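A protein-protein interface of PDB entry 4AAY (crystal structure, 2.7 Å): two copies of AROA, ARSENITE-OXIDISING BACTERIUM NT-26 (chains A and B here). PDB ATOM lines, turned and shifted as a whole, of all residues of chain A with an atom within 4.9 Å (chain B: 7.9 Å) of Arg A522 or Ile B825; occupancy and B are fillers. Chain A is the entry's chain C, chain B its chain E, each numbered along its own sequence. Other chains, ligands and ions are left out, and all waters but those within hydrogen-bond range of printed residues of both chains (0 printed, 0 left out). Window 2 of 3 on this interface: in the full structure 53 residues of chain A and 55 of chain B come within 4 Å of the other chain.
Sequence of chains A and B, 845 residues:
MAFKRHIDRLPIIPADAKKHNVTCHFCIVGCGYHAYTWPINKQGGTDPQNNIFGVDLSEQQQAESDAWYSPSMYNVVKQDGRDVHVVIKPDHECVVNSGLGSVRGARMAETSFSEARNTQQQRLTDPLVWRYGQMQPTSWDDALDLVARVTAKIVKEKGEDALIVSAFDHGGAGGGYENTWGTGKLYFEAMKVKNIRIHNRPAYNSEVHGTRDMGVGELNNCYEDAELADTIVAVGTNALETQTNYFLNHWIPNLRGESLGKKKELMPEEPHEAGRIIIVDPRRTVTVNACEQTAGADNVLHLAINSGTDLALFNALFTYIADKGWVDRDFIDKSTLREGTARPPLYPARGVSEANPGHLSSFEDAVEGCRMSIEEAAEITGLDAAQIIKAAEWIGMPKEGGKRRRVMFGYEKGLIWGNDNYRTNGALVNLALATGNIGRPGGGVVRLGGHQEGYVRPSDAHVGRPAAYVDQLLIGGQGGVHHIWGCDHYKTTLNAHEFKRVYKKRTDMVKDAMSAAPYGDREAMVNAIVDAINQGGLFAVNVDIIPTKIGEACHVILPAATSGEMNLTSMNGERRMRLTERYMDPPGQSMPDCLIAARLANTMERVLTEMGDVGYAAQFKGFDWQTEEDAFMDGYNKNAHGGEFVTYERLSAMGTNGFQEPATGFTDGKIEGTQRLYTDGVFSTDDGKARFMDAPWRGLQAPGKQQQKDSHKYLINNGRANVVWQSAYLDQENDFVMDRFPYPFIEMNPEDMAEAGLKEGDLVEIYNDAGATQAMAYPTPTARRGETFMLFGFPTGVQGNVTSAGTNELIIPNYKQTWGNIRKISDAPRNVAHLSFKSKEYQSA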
ATOM      1  N   ARG A 131      -3.820  -1.765   9.911  1.00  0.00           N
ATOM      2  CA  ARG A 131      -3.558  -1.430  11.299  1.00  0.00           C
ATOM      3  C   ARG A 131      -2.352  -0.534  11.447  1.00  0.00           C
ATOM      4  O   ARG A 131      -1.496  -0.507  10.591  1.00  0.00           O
ATOM      5  CB  ARG A 131      -3.360  -2.679  12.154  1.00  0.00           C
ATOM      6  CG  ARG A 131      -2.292  -3.651  11.654  1.00  0.00           C
ATOM      7  CD  ARG A 131      -2.126  -4.763  12.676  1.00  0.00           C
ATOM      8  NE  ARG A 131      -1.031  -5.686  12.395  1.00  0.00           N
ATOM      9  CZ  ARG A 131      -1.167  -6.987  12.150  1.00  0.00           C
ATOM     10  NH1 ARG A 131      -2.360  -7.566  12.102  1.00  0.00           N
ATOM     11  NH2 ARG A 131      -0.089  -7.729  11.942  1.00  0.00           N
ATOM     12  N   TYR A 132      -2.302   0.201  12.546  1.00  0.00           N
ATOM     13  CA  TYR A 132      -1.211   1.117  12.816  1.00  0.00           C
ATOM     14  C   TYR A 132      -1.078   2.208  11.754  1.00  0.00           C
ATOM     15  O   TYR A 132       0.023   2.754  11.526  1.00  0.00           O
ATOM     16  CB  TYR A 132       0.098   0.347  12.925  1.00  0.00           C
ATOM     17  CG  TYR A 132       0.023  -0.859  13.806  1.00  0.00           C
ATOM     18  CD1 TYR A 132      -0.560  -0.786  15.080  1.00  0.00           C
ATOM     19  CD2 TYR A 132       0.556  -2.074  13.398  1.00  0.00           C
ATOM     20  CE1 TYR A 132      -0.626  -1.895  15.907  1.00  0.00           C
ATOM     21  CE2 TYR A 132       0.508  -3.179  14.229  1.00  0.00           C
ATOM     22  CZ  TYR A 132      -0.083  -3.079  15.484  1.00  0.00           C
ATOM     23  OH  TYR A 132      -0.127  -4.178  16.303  1.00  0.00           O
ATOM     24  N   THR A 138       0.949  -9.780   7.702  1.00  0.00           N
ATOM     25  CA  THR A 138       0.770 -10.589   8.891  1.00  0.00           C
ATOM     26  C   THR A 138       0.677 -12.048   8.497  1.00  0.00           C
ATOM     27  O   THR A 138       0.814 -12.382   7.321  1.00  0.00           O
ATOM     28  CB  THR A 138      -0.488 -10.141   9.684  1.00  0.00           C
ATOM     29  OG1 THR A 138      -0.483 -10.749  10.986  1.00  0.00           O
ATOM     30  CG2 THR A 138      -1.757 -10.481   8.949  1.00  0.00           C
ATOM     31  N   ASP A 142      -3.504 -14.975  12.060  1.00  0.00           N
ATOM     32  CA  ASP A 142      -3.953 -13.651  12.473  1.00  0.00           C
ATOM     33  C   ASP A 142      -5.053 -13.125  11.558  1.00  0.00           C
ATOM     34  O   ASP A 142      -6.067 -12.661  12.022  1.00  0.00           O
ATOM     35  CB  ASP A 142      -2.774 -12.671  12.485  1.00  0.00           C
ATOM     36  CG  ASP A 142      -3.175 -11.285  12.928  1.00  0.00           C
ATOM     37  OD1 ASP A 142      -3.969 -11.184  13.877  1.00  0.00           O
ATOM     38  OD2 ASP A 142      -2.700 -10.289  12.335  1.00  0.00           O
ATOM     39  N   ASP A 145      -8.333 -15.103  11.686  1.00  0.00           N
ATOM     40  CA  ASP A 145      -8.990 -14.882  12.980  1.00  0.00           C
ATOM     41  C   ASP A 145      -9.774 -13.585  12.944  1.00  0.00           C
ATOM     42  O   ASP A 145     -10.901 -13.538  13.383  1.00  0.00           O
ATOM     43  CB  ASP A 145      -7.975 -14.868  14.120  1.00  0.00           C
ATOM     44  CG  ASP A 145      -8.625 -14.732  15.495  1.00  0.00           C
ATOM     45  OD1 ASP A 145      -9.283 -15.711  15.934  1.00  0.00           O
ATOM     46  OD2 ASP A 145      -8.458 -13.668  16.161  1.00  0.00           O
ATOM     47  N   ARG A 149     -13.852 -13.474  13.256  1.00  0.00           N
ATOM     48  CA  ARG A 149     -14.450 -12.820  14.408  1.00  0.00           C
ATOM     49  C   ARG A 149     -15.412 -11.715  14.028  1.00  0.00           C
ATOM     50  O   ARG A 149     -16.499 -11.626  14.597  1.00  0.00           O
ATOM     51  CB  ARG A 149     -13.393 -12.222  15.310  1.00  0.00           C
ATOM     52  CG  ARG A 149     -12.546 -13.244  16.039  1.00  0.00           C
ATOM     53  CD  ARG A 149     -12.212 -12.694  17.406  1.00  0.00           C
ATOM     54  NE  ARG A 149     -10.842 -12.950  17.841  1.00  0.00           N
ATOM     55  CZ  ARG A 149     -10.355 -12.516  19.001  1.00  0.00           C
ATOM     56  NH1 ARG A 149     -11.124 -11.818  19.828  1.00  0.00           N
ATOM     57  NH2 ARG A 149      -9.094 -12.777  19.338  1.00  0.00           N
ATOM     58  N   PRO A 518      -6.594  -0.379  19.789  1.00  0.00           N
ATOM     59  CA  PRO A 518      -5.439  -1.234  19.995  1.00  0.00           C
ATOM     60  C   PRO A 518      -5.652  -2.584  19.315  1.00  0.00           C
ATOM     61  O   PRO A 518      -6.655  -3.251  19.575  1.00  0.00           O
ATOM     62  CB  PRO A 518      -5.396  -1.388  21.518  1.00  0.00           C
ATOM     63  CG  PRO A 518      -6.814  -1.225  21.971  1.00  0.00           C
ATOM     64  CD  PRO A 518      -7.573  -0.497  20.889  1.00  0.00           C
ATOM     65  N   TYR A 519      -4.737  -2.967  18.432  1.00  0.00           N
ATOM     66  CA  TYR A 519      -4.857  -4.246  17.705  1.00  0.00           C
ATOM     67  C   TYR A 519      -4.486  -5.449  18.586  1.00  0.00           C
ATOM     68  O   TYR A 519      -5.134  -6.490  18.539  1.00  0.00           O
ATOM     69  CB  TYR A 519      -3.993  -4.250  16.440  1.00  0.00           C
ATOM     70  CG  TYR A 519      -4.237  -5.471  15.584  1.00  0.00           C
ATOM     71  CD1 TYR A 519      -5.279  -5.500  14.680  1.00  0.00           C
ATOM     72  CD2 TYR A 519      -3.450  -6.602  15.710  1.00  0.00           C
ATOM     73  CE1 TYR A 519      -5.531  -6.611  13.899  1.00  0.00           C
ATOM     74  CE2 TYR A 519      -3.697  -7.730  14.943  1.00  0.00           C
ATOM     75  CZ  TYR A 519      -4.750  -7.730  14.040  1.00  0.00           C
ATOM     76  OH  TYR A 519      -5.010  -8.847  13.265  1.00  0.00           O
ATOM     77  N   GLY A 520      -3.423  -5.304  19.370  1.00  0.00           N
ATOM     78  CA  GLY A 520      -2.938  -6.384  20.225  1.00  0.00           C
ATOM     79  C   GLY A 520      -3.953  -6.888  21.233  1.00  0.00           C
ATOM     80  O   GLY A 520      -3.812  -7.993  21.743  1.00  0.00           O
ATOM     81  N   ASP A 521      -4.932  -6.042  21.556  1.00  0.00           N
ATOM     82  CA  ASP A 521      -6.140  -6.440  22.280  1.00  0.00           C
ATOM     83  C   ASP A 521      -7.239  -6.634  21.238  1.00  0.00           C
ATOM     84  O   ASP A 521      -7.973  -5.707  20.914  1.00  0.00           O
ATOM     85  CB  ASP A 521      -6.539  -5.368  23.301  1.00  0.00           C
ATOM     86  CG  ASP A 521      -7.841  -5.689  24.026  1.00  0.00           C
ATOM     87  OD1 ASP A 521      -8.517  -6.694  23.677  1.00  0.00           O
ATOM     88  OD2 ASP A 521      -8.184  -4.934  24.959  1.00  0.00           O
ATOM     89  N   ARG A 522      -7.359  -7.856  20.735  1.00  0.00           N
ATOM     90  CA  ARG A 522      -8.195  -8.104  19.578  1.00  0.00           C
ATOM     91  C   ARG A 522      -9.687  -7.954  19.827  1.00  0.00           C
ATOM     92  O   ARG A 522     -10.430  -7.587  18.917  1.00  0.00           O
ATOM     93  CB  ARG A 522      -7.868  -9.443  18.925  1.00  0.00           C
ATOM     94  CG  ARG A 522      -7.253  -9.231  17.554  1.00  0.00           C
ATOM     95  CD  ARG A 522      -6.892 -10.522  16.866  1.00  0.00           C
ATOM     96  NE  ARG A 522      -5.518 -10.587  16.372  1.00  0.00           N
ATOM     97  CZ  ARG A 522      -4.436 -10.603  17.148  1.00  0.00           C
ATOM     98  NH1 ARG A 522      -4.528 -10.506  18.461  1.00  0.00           N
ATOM     99  NH2 ARG A 522      -3.241 -10.699  16.594  1.00  0.00           N
ATOM    100  N   GLU A 523     -10.134  -8.226  21.045  1.00  0.00           N
ATOM    101  CA  GLU A 523     -11.550  -8.077  21.359  1.00  0.00           C
ATOM    102  C   GLU A 523     -11.964  -6.598  21.264  1.00  0.00           C
ATOM    103  O   GLU A 523     -13.044  -6.279  20.773  1.00  0.00           O
ATOM    104  CB  GLU A 523     -11.877  -8.690  22.731  1.00  0.00           C
ATOM    105  CG  GLU A 523     -13.367  -8.854  23.049  1.00  0.00           C
ATOM    106  CD  GLU A 523     -14.122  -9.872  22.166  1.00  0.00           C
ATOM    107  OE1 GLU A 523     -13.692 -10.188  21.022  1.00  0.00           O
ATOM    108  OE2 GLU A 523     -15.193 -10.348  22.617  1.00  0.00           O
ATOM    109  N   ALA A 524     -11.089  -5.696  21.690  1.00  0.00           N
ATOM    110  CA  ALA A 524     -11.381  -4.260  21.598  1.00  0.00           C
ATOM    111  C   ALA A 524     -11.377  -3.798  20.126  1.00  0.00           C
ATOM    112  O   ALA A 524     -12.186  -2.975  19.722  1.00  0.00           O
ATOM    113  CB  ALA A 524     -10.404  -3.452  22.429  1.00  0.00           C
ATOM    114  N   MET A 525     -10.474  -4.361  19.330  1.00  0.00           N
ATOM    115  CA  MET A 525     -10.408  -4.067  17.892  1.00  0.00           C
ATOM    116  C   MET A 525     -11.684  -4.481  17.162  1.00  0.00           C
ATOM    117  O   MET A 525     -12.187  -3.748  16.320  1.00  0.00           O
ATOM    118  CB  MET A 525      -9.187  -4.759  17.266  1.00  0.00           C
ATOM    119  CG  MET A 525      -9.063  -4.611  15.757  1.00  0.00           C
ATOM    120  SD  MET A 525      -8.954  -2.890  15.236  1.00  0.00           S
ATOM    121  CE  MET A 525      -7.348  -2.388  15.883  1.00  0.00           C
ATOM    122  N   VAL A 526     -12.204  -5.652  17.496  1.00  0.00           N
ATOM    123  CA  VAL A 526     -13.394  -6.181  16.834  1.00  0.00           C
ATOM    124  C   VAL A 526     -14.627  -5.411  17.251  1.00  0.00           C
ATOM    125  O   VAL A 526     -15.488  -5.122  16.422  1.00  0.00           O
ATOM    126  CB  VAL A 526     -13.567  -7.693  17.094  1.00  0.00           C
ATOM    127  CG1 VAL A 526     -14.962  -8.157  16.667  1.00  0.00           C
ATOM    128  CG2 VAL A 526     -12.477  -8.464  16.350  1.00  0.00           C
ATOM    129  N   LEU B 758       8.046 -15.325  24.054  1.00  0.00           N
ATOM    130  CA  LEU B 758       8.308 -15.055  22.634  1.00  0.00           C
ATOM    131  C   LEU B 758       9.409 -15.938  22.069  1.00  0.00           C
ATOM    132  O   LEU B 758      10.377 -16.257  22.757  1.00  0.00           O
ATOM    133  CB  LEU B 758       8.708 -13.601  22.423  1.00  0.00           C
ATOM    134  CG  LEU B 758       7.719 -12.565  22.939  1.00  0.00           C
ATOM    135  CD1 LEU B 758       8.376 -11.191  22.974  1.00  0.00           C
ATOM    136  CD2 LEU B 758       6.458 -12.588  22.075  1.00  0.00           C
ATOM    137  N   ASP B 762       8.654 -14.374  16.068  1.00  0.00           N
ATOM    138  CA  ASP B 762       7.317 -13.962  16.500  1.00  0.00           C
ATOM    139  C   ASP B 762       7.078 -12.525  16.120  1.00  0.00           C
ATOM    140  O   ASP B 762       7.963 -11.695  16.151  1.00  0.00           O
ATOM    141  CB  ASP B 762       7.109 -14.149  18.006  1.00  0.00           C
ATOM    142  CG  ASP B 762       6.856 -15.585  18.380  1.00  0.00           C
ATOM    143  OD1 ASP B 762       6.701 -16.415  17.458  1.00  0.00           O
ATOM    144  OD2 ASP B 762       6.816 -15.898  19.594  1.00  0.00           O
ATOM    145  N   LEU B 763       5.851 -12.256  15.733  1.00  0.00           N
ATOM    146  CA  LEU B 763       5.433 -10.927  15.336  1.00  0.00           C
ATOM    147  C   LEU B 763       4.839 -10.289  16.587  1.00  0.00           C
ATOM    148  O   LEU B 763       3.882 -10.810  17.161  1.00  0.00           O
ATOM    149  CB  LEU B 763       4.416 -11.056  14.196  1.00  0.00           C
ATOM    150  CG  LEU B 763       4.108  -9.843  13.349  1.00  0.00           C
ATOM    151  CD1 LEU B 763       5.426  -9.418  12.721  1.00  0.00           C
ATOM    152  CD2 LEU B 763       3.074 -10.146  12.264  1.00  0.00           C
ATOM    153  N   VAL B 764       5.419  -9.175  17.018  1.00  0.00           N
ATOM    154  CA  VAL B 764       5.036  -8.535  18.281  1.00  0.00           C
ATOM    155  C   VAL B 764       4.557  -7.113  18.080  1.00  0.00           C
ATOM    156  O   VAL B 764       5.019  -6.409  17.178  1.00  0.00           O
ATOM    157  CB  VAL B 764       6.197  -8.502  19.281  1.00  0.00           C
ATOM    158  CG1 VAL B 764       6.611  -9.923  19.624  1.00  0.00           C
ATOM    159  CG2 VAL B 764       7.388  -7.730  18.721  1.00  0.00           C
ATOM    160  N   GLU B 765       3.582  -6.720  18.894  1.00  0.00           N
ATOM    161  CA  GLU B 765       3.125  -5.333  18.958  1.00  0.00           C
ATOM    162  C   GLU B 765       3.966  -4.607  19.992  1.00  0.00           C
ATOM    163  O   GLU B 765       4.104  -5.072  21.112  1.00  0.00           O
ATOM    164  CB  GLU B 765       1.647  -5.241  19.336  1.00  0.00           C
ATOM    165  CG  GLU B 765       1.090  -3.807  19.407  1.00  0.00           C
ATOM    166  CD  GLU B 765      -0.429  -3.767  19.644  1.00  0.00           C
ATOM    167  OE1 GLU B 765      -0.864  -3.944  20.822  1.00  0.00           O
ATOM    168  OE2 GLU B 765      -1.185  -3.553  18.657  1.00  0.00           O
ATOM    169  N   ILE B 766       4.534  -3.478  19.591  1.00  0.00           N
ATOM    170  CA  ILE B 766       5.175  -2.550  20.514  1.00  0.00           C
ATOM    171  C   ILE B 766       4.147  -1.457  20.751  1.00  0.00           C
ATOM    172  O   ILE B 766       3.606  -0.935  19.790  1.00  0.00           O
ATOM    173  CB  ILE B 766       6.427  -1.891  19.912  1.00  0.00           C
ATOM    174  CG1 ILE B 766       7.191  -2.863  18.967  1.00  0.00           C
ATOM    175  CG2 ILE B 766       7.286  -1.282  21.010  1.00  0.00           C
ATOM    176  CD1 ILE B 766       7.508  -4.204  19.549  1.00  0.00           C
ATOM    177  N   THR B 773       2.688  -0.399  17.015  1.00  0.00           N
ATOM    178  CA  THR B 773       3.284  -0.853  15.765  1.00  0.00           C
ATOM    179  C   THR B 773       3.704  -2.314  15.886  1.00  0.00           C
ATOM    180  O   THR B 773       3.538  -2.929  16.938  1.00  0.00           O
ATOM    181  CB  THR B 773       4.504   0.019  15.404  1.00  0.00           C
ATOM    182  OG1 THR B 773       4.877  -0.211  14.049  1.00  0.00           O
ATOM    183  CG2 THR B 773       5.698  -0.310  16.310  1.00  0.00           C
ATOM    184  N   GLN B 774       4.288  -2.853  14.829  1.00  0.00           N
ATOM    185  CA  GLN B 774       4.680  -4.259  14.821  1.00  0.00           C
ATOM    186  C   GLN B 774       6.141  -4.439  14.424  1.00  0.00           C
ATOM    187  O   GLN B 774       6.715  -3.598  13.747  1.00  0.00           O
ATOM    188  CB  GLN B 774       3.776  -5.052  13.874  1.00  0.00           C
ATOM    189  CG  GLN B 774       3.808  -4.631  12.410  1.00  0.00           C
ATOM    190  CD  GLN B 774       2.883  -5.486  11.551  1.00  0.00           C
ATOM    191  OE1 GLN B 774       1.809  -5.883  11.990  1.00  0.00           O
ATOM    192  NE2 GLN B 774       3.300  -5.765  10.318  1.00  0.00           N
ATOM    193  N   ALA B 775       6.732  -5.545  14.858  1.00  0.00           N
ATOM    194  CA  ALA B 775       8.103  -5.890  14.475  1.00  0.00           C
ATOM    195  C   ALA B 775       8.317  -7.368  14.694  1.00  0.00           C
ATOM    196  O   ALA B 775       7.491  -8.045  15.308  1.00  0.00           O
ATOM    197  CB  ALA B 775       9.127  -5.084  15.270  1.00  0.00           C
ATOM    198  N   ILE B 822       5.701  -4.542  25.121  1.00  0.00           N
ATOM    199  CA  ILE B 822       5.713  -5.492  24.007  1.00  0.00           C
ATOM    200  C   ILE B 822       4.790  -6.667  24.296  1.00  0.00           C
ATOM    201  O   ILE B 822       4.797  -7.207  25.387  1.00  0.00           O
ATOM    202  CB  ILE B 822       7.134  -6.006  23.735  1.00  0.00           C
ATOM    203  CG1 ILE B 822       8.041  -4.827  23.331  1.00  0.00           C
ATOM    204  CG2 ILE B 822       7.123  -7.054  22.635  1.00  0.00           C
ATOM    205  CD1 ILE B 822       9.513  -5.176  23.214  1.00  0.00           C
ATOM    206  N   ARG B 823       3.980  -7.041  23.316  1.00  0.00           N
ATOM    207  CA  ARG B 823       3.154  -8.252  23.423  1.00  0.00           C
ATOM    208  C   ARG B 823       2.979  -8.910  22.066  1.00  0.00           C
ATOM    209  O   ARG B 823       3.073  -8.264  21.046  1.00  0.00           O
ATOM    210  CB  ARG B 823       1.781  -7.957  24.038  1.00  0.00           C
ATOM    211  CG  ARG B 823       0.910  -7.054  23.193  1.00  0.00           C
ATOM    212  CD  ARG B 823      -0.286  -6.561  23.971  1.00  0.00           C
ATOM    213  NE  ARG B 823      -0.989  -5.511  23.236  1.00  0.00           N
ATOM    214  CZ  ARG B 823      -2.005  -4.786  23.709  1.00  0.00           C
ATOM    215  NH1 ARG B 823      -2.448  -4.988  24.945  1.00  0.00           N
ATOM    216  NH2 ARG B 823      -2.587  -3.862  22.938  1.00  0.00           N
ATOM    217  N   LYS B 824       2.693 -10.204  22.084  1.00  0.00           N
ATOM    218  CA  LYS B 824       2.689 -11.019  20.884  1.00  0.00           C
ATOM    219  C   LYS B 824       1.445 -10.784  20.061  1.00  0.00           C
ATOM    220  O   LYS B 824       0.342 -10.821  20.596  1.00  0.00           O
ATOM    221  CB  LYS B 824       2.768 -12.479  21.300  1.00  0.00           C
ATOM    222  CG  LYS B 824       2.853 -13.500  20.187  1.00  0.00           C
ATOM    223  CD  LYS B 824       3.357 -14.809  20.785  1.00  0.00           C
ATOM    224  CE  LYS B 824       2.722 -16.037  20.157  1.00  0.00           C
ATOM    225  NZ  LYS B 824       2.924 -17.301  20.911  1.00  0.00           N
ATOM    226  N   ILE B 825       1.623 -10.548  18.768  1.00  0.00           N
ATOM    227  CA  ILE B 825       0.502 -10.486  17.829  1.00  0.00           C
ATOM    228  C   ILE B 825       0.262 -11.854  17.190  1.00  0.00           C
ATOM    229  O   ILE B 825      -0.871 -12.293  17.051  1.00  0.00           O
ATOM    230  CB  ILE B 825       0.779  -9.529  16.667  1.00  0.00           C
ATOM    231  CG1 ILE B 825       0.912  -8.101  17.135  1.00  0.00           C
ATOM    232  CG2 ILE B 825      -0.352  -9.579  15.655  1.00  0.00           C
ATOM    233  CD1 ILE B 825       1.421  -7.209  16.022  1.00  0.00           C
ATOM    234  N   SER B 826       1.341 -12.502  16.771  1.00  0.00           N
ATOM    235  CA  SER B 826       1.253 -13.779  16.061  1.00  0.00           C
ATOM    236  C   SER B 826       2.496 -14.646  16.272  1.00  0.00           C
ATOM    237  O   SER B 826       3.594 -14.125  16.433  1.00  0.00           O
ATOM    238  CB  SER B 826       1.057 -13.526  14.558  1.00  0.00           C
ATOM    239  OG  SER B 826       1.217 -14.715  13.800  1.00  0.00           O
ATOM    240  N   ASP B 827       2.303 -15.964  16.268  1.00  0.00           N
ATOM    241  CA  ASP B 827       3.412 -16.904  16.117  1.00  0.00           C
ATOM    242  C   ASP B 827       4.168 -16.549  14.839  1.00  0.00           C
ATOM    243  O   ASP B 827       3.585 -16.005  13.905  1.00  0.00           O
ATOM    244  CB  ASP B 827       2.920 -18.347  15.996  1.00  0.00           C
ATOM    245  CG  ASP B 827       2.365 -18.905  17.301  1.00  0.00           C
ATOM    246  OD1 ASP B 827       2.801 -18.468  18.396  1.00  0.00           O
ATOM    247  OD2 ASP B 827       1.510 -19.817  17.232  1.00  0.00           O
ATOM    248  N   ALA B 828       5.472 -16.820  14.823  1.00  0.00           N
ATOM    249  CA  ALA B 828       6.316 -16.524  13.655  1.00  0.00           C
ATOM    250  C   ALA B 828       5.617 -16.928  12.349  1.00  0.00           C
ATOM    251  O   ALA B 828       5.300 -18.093  12.162  1.00  0.00           O
ATOM    252  CB  ALA B 828       7.658 -17.234  13.769  1.00  0.00           C
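OE2 of Glu B765 sits at hydrogen-bond distance from N of Gly A520 (2.9 Å).
The backbone NH (N) of Asp A521 sits close to the guanidinium group (NH2) of Arg B823, at 3.5 Å.
NH2 of Arg A131 sits at hydrogen-bond distance from OE1 of Gln B774.
The guanidinium group (NH2) of Arg A522 sits at hydrogen-bond distance from the backbone carbonyl oxygen (O) of Ile B825 (2.9 Å).
OH of Tyr A132 sits at hydrogen-bond distance from OE2 of Glu B765, 2.7 Å away.
N of Leu B763 sits at hydrogen-bond distance from O of Ser B826 (3.0 Å).
The backbone carbonyl oxygen (O) of Leu B763 is in hydrogen-bond range of the backbone NH (N) of Ile B825.
The guanidinium group (NH1) of Arg A131 sits close to the side-chain hydroxyl (OH) of Tyr A519, at 3.2 Å.
The side-chain hydroxyl of Thr A138 sits at hydrogen-bond distance from the side-chain carboxylate of Asp A142 (2.6 Å).
The backbone NH (N) of Ala A524 is in hydrogen-bond range of the side-chain carboxylate (OD1) of Asp A521 (3.4 Å).
The side-chain carboxylate of Glu B765 is in salt-bridge range of the guanidinium group of Arg B823 (2.7 Å).
Among the printed residues, merely in contact across the chains: Arg A131 with Leu B763 (3.99 Å), Tyr A132 with Thr B773 (3.7 Å), Tyr A132 with Gln B774 (3.7 Å), Tyr A132 with Ile B825 (3.4 Å), Thr A138 with Leu B763 (3.8 Å), Tyr A519 with Glu B765 (3.6 Å), Tyr A519 with Ile B825 (3.9 Å) and Gly A520 with Arg B823 (3.7 Å).
Arg A522 touches just one residue of chain B: Ile B825.
Ile B825 touches just these residues of chain A: Tyr A132 (3.4 Å), Tyr A519 (3.9 Å) and Arg A522 (2.9 Å).
Printed residues of chain A within 4 Å of Glu B765: Tyr A132 (2.7 Å), Tyr A519 (3.6 Å) and Gly A520 (2.9 Å).
Printed residues of chain B within 4 Å of Tyr A519: Glu B765 (3.6 Å) and Ile B825 (3.9 Å).
Of the printed residues of chain A, Thr B773 touches Tyr A132.
The nearest printed residue of chain B that does not touch Arg A131 is Ile B825 (4.2 Å).
Of the 15 printed residues of chain A, 7 touch a printed residue of chain B.
Printed residues of chain A that touch a printed residue of chain B: Arg A131, Tyr A132, Thr A138, Tyr A519, Gly A520, Asp A521 and Arg A522.
Hydrophobic or aromatic side chains of chain A that line the printed part of chain B: Tyr A132 and Tyr A519.
Along chain B the printed residues that touch a printed residue of chain A span positions 763 to 825.
Among the printed residues, 13 pairs touch across the chains.
No position is printed for both chains.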
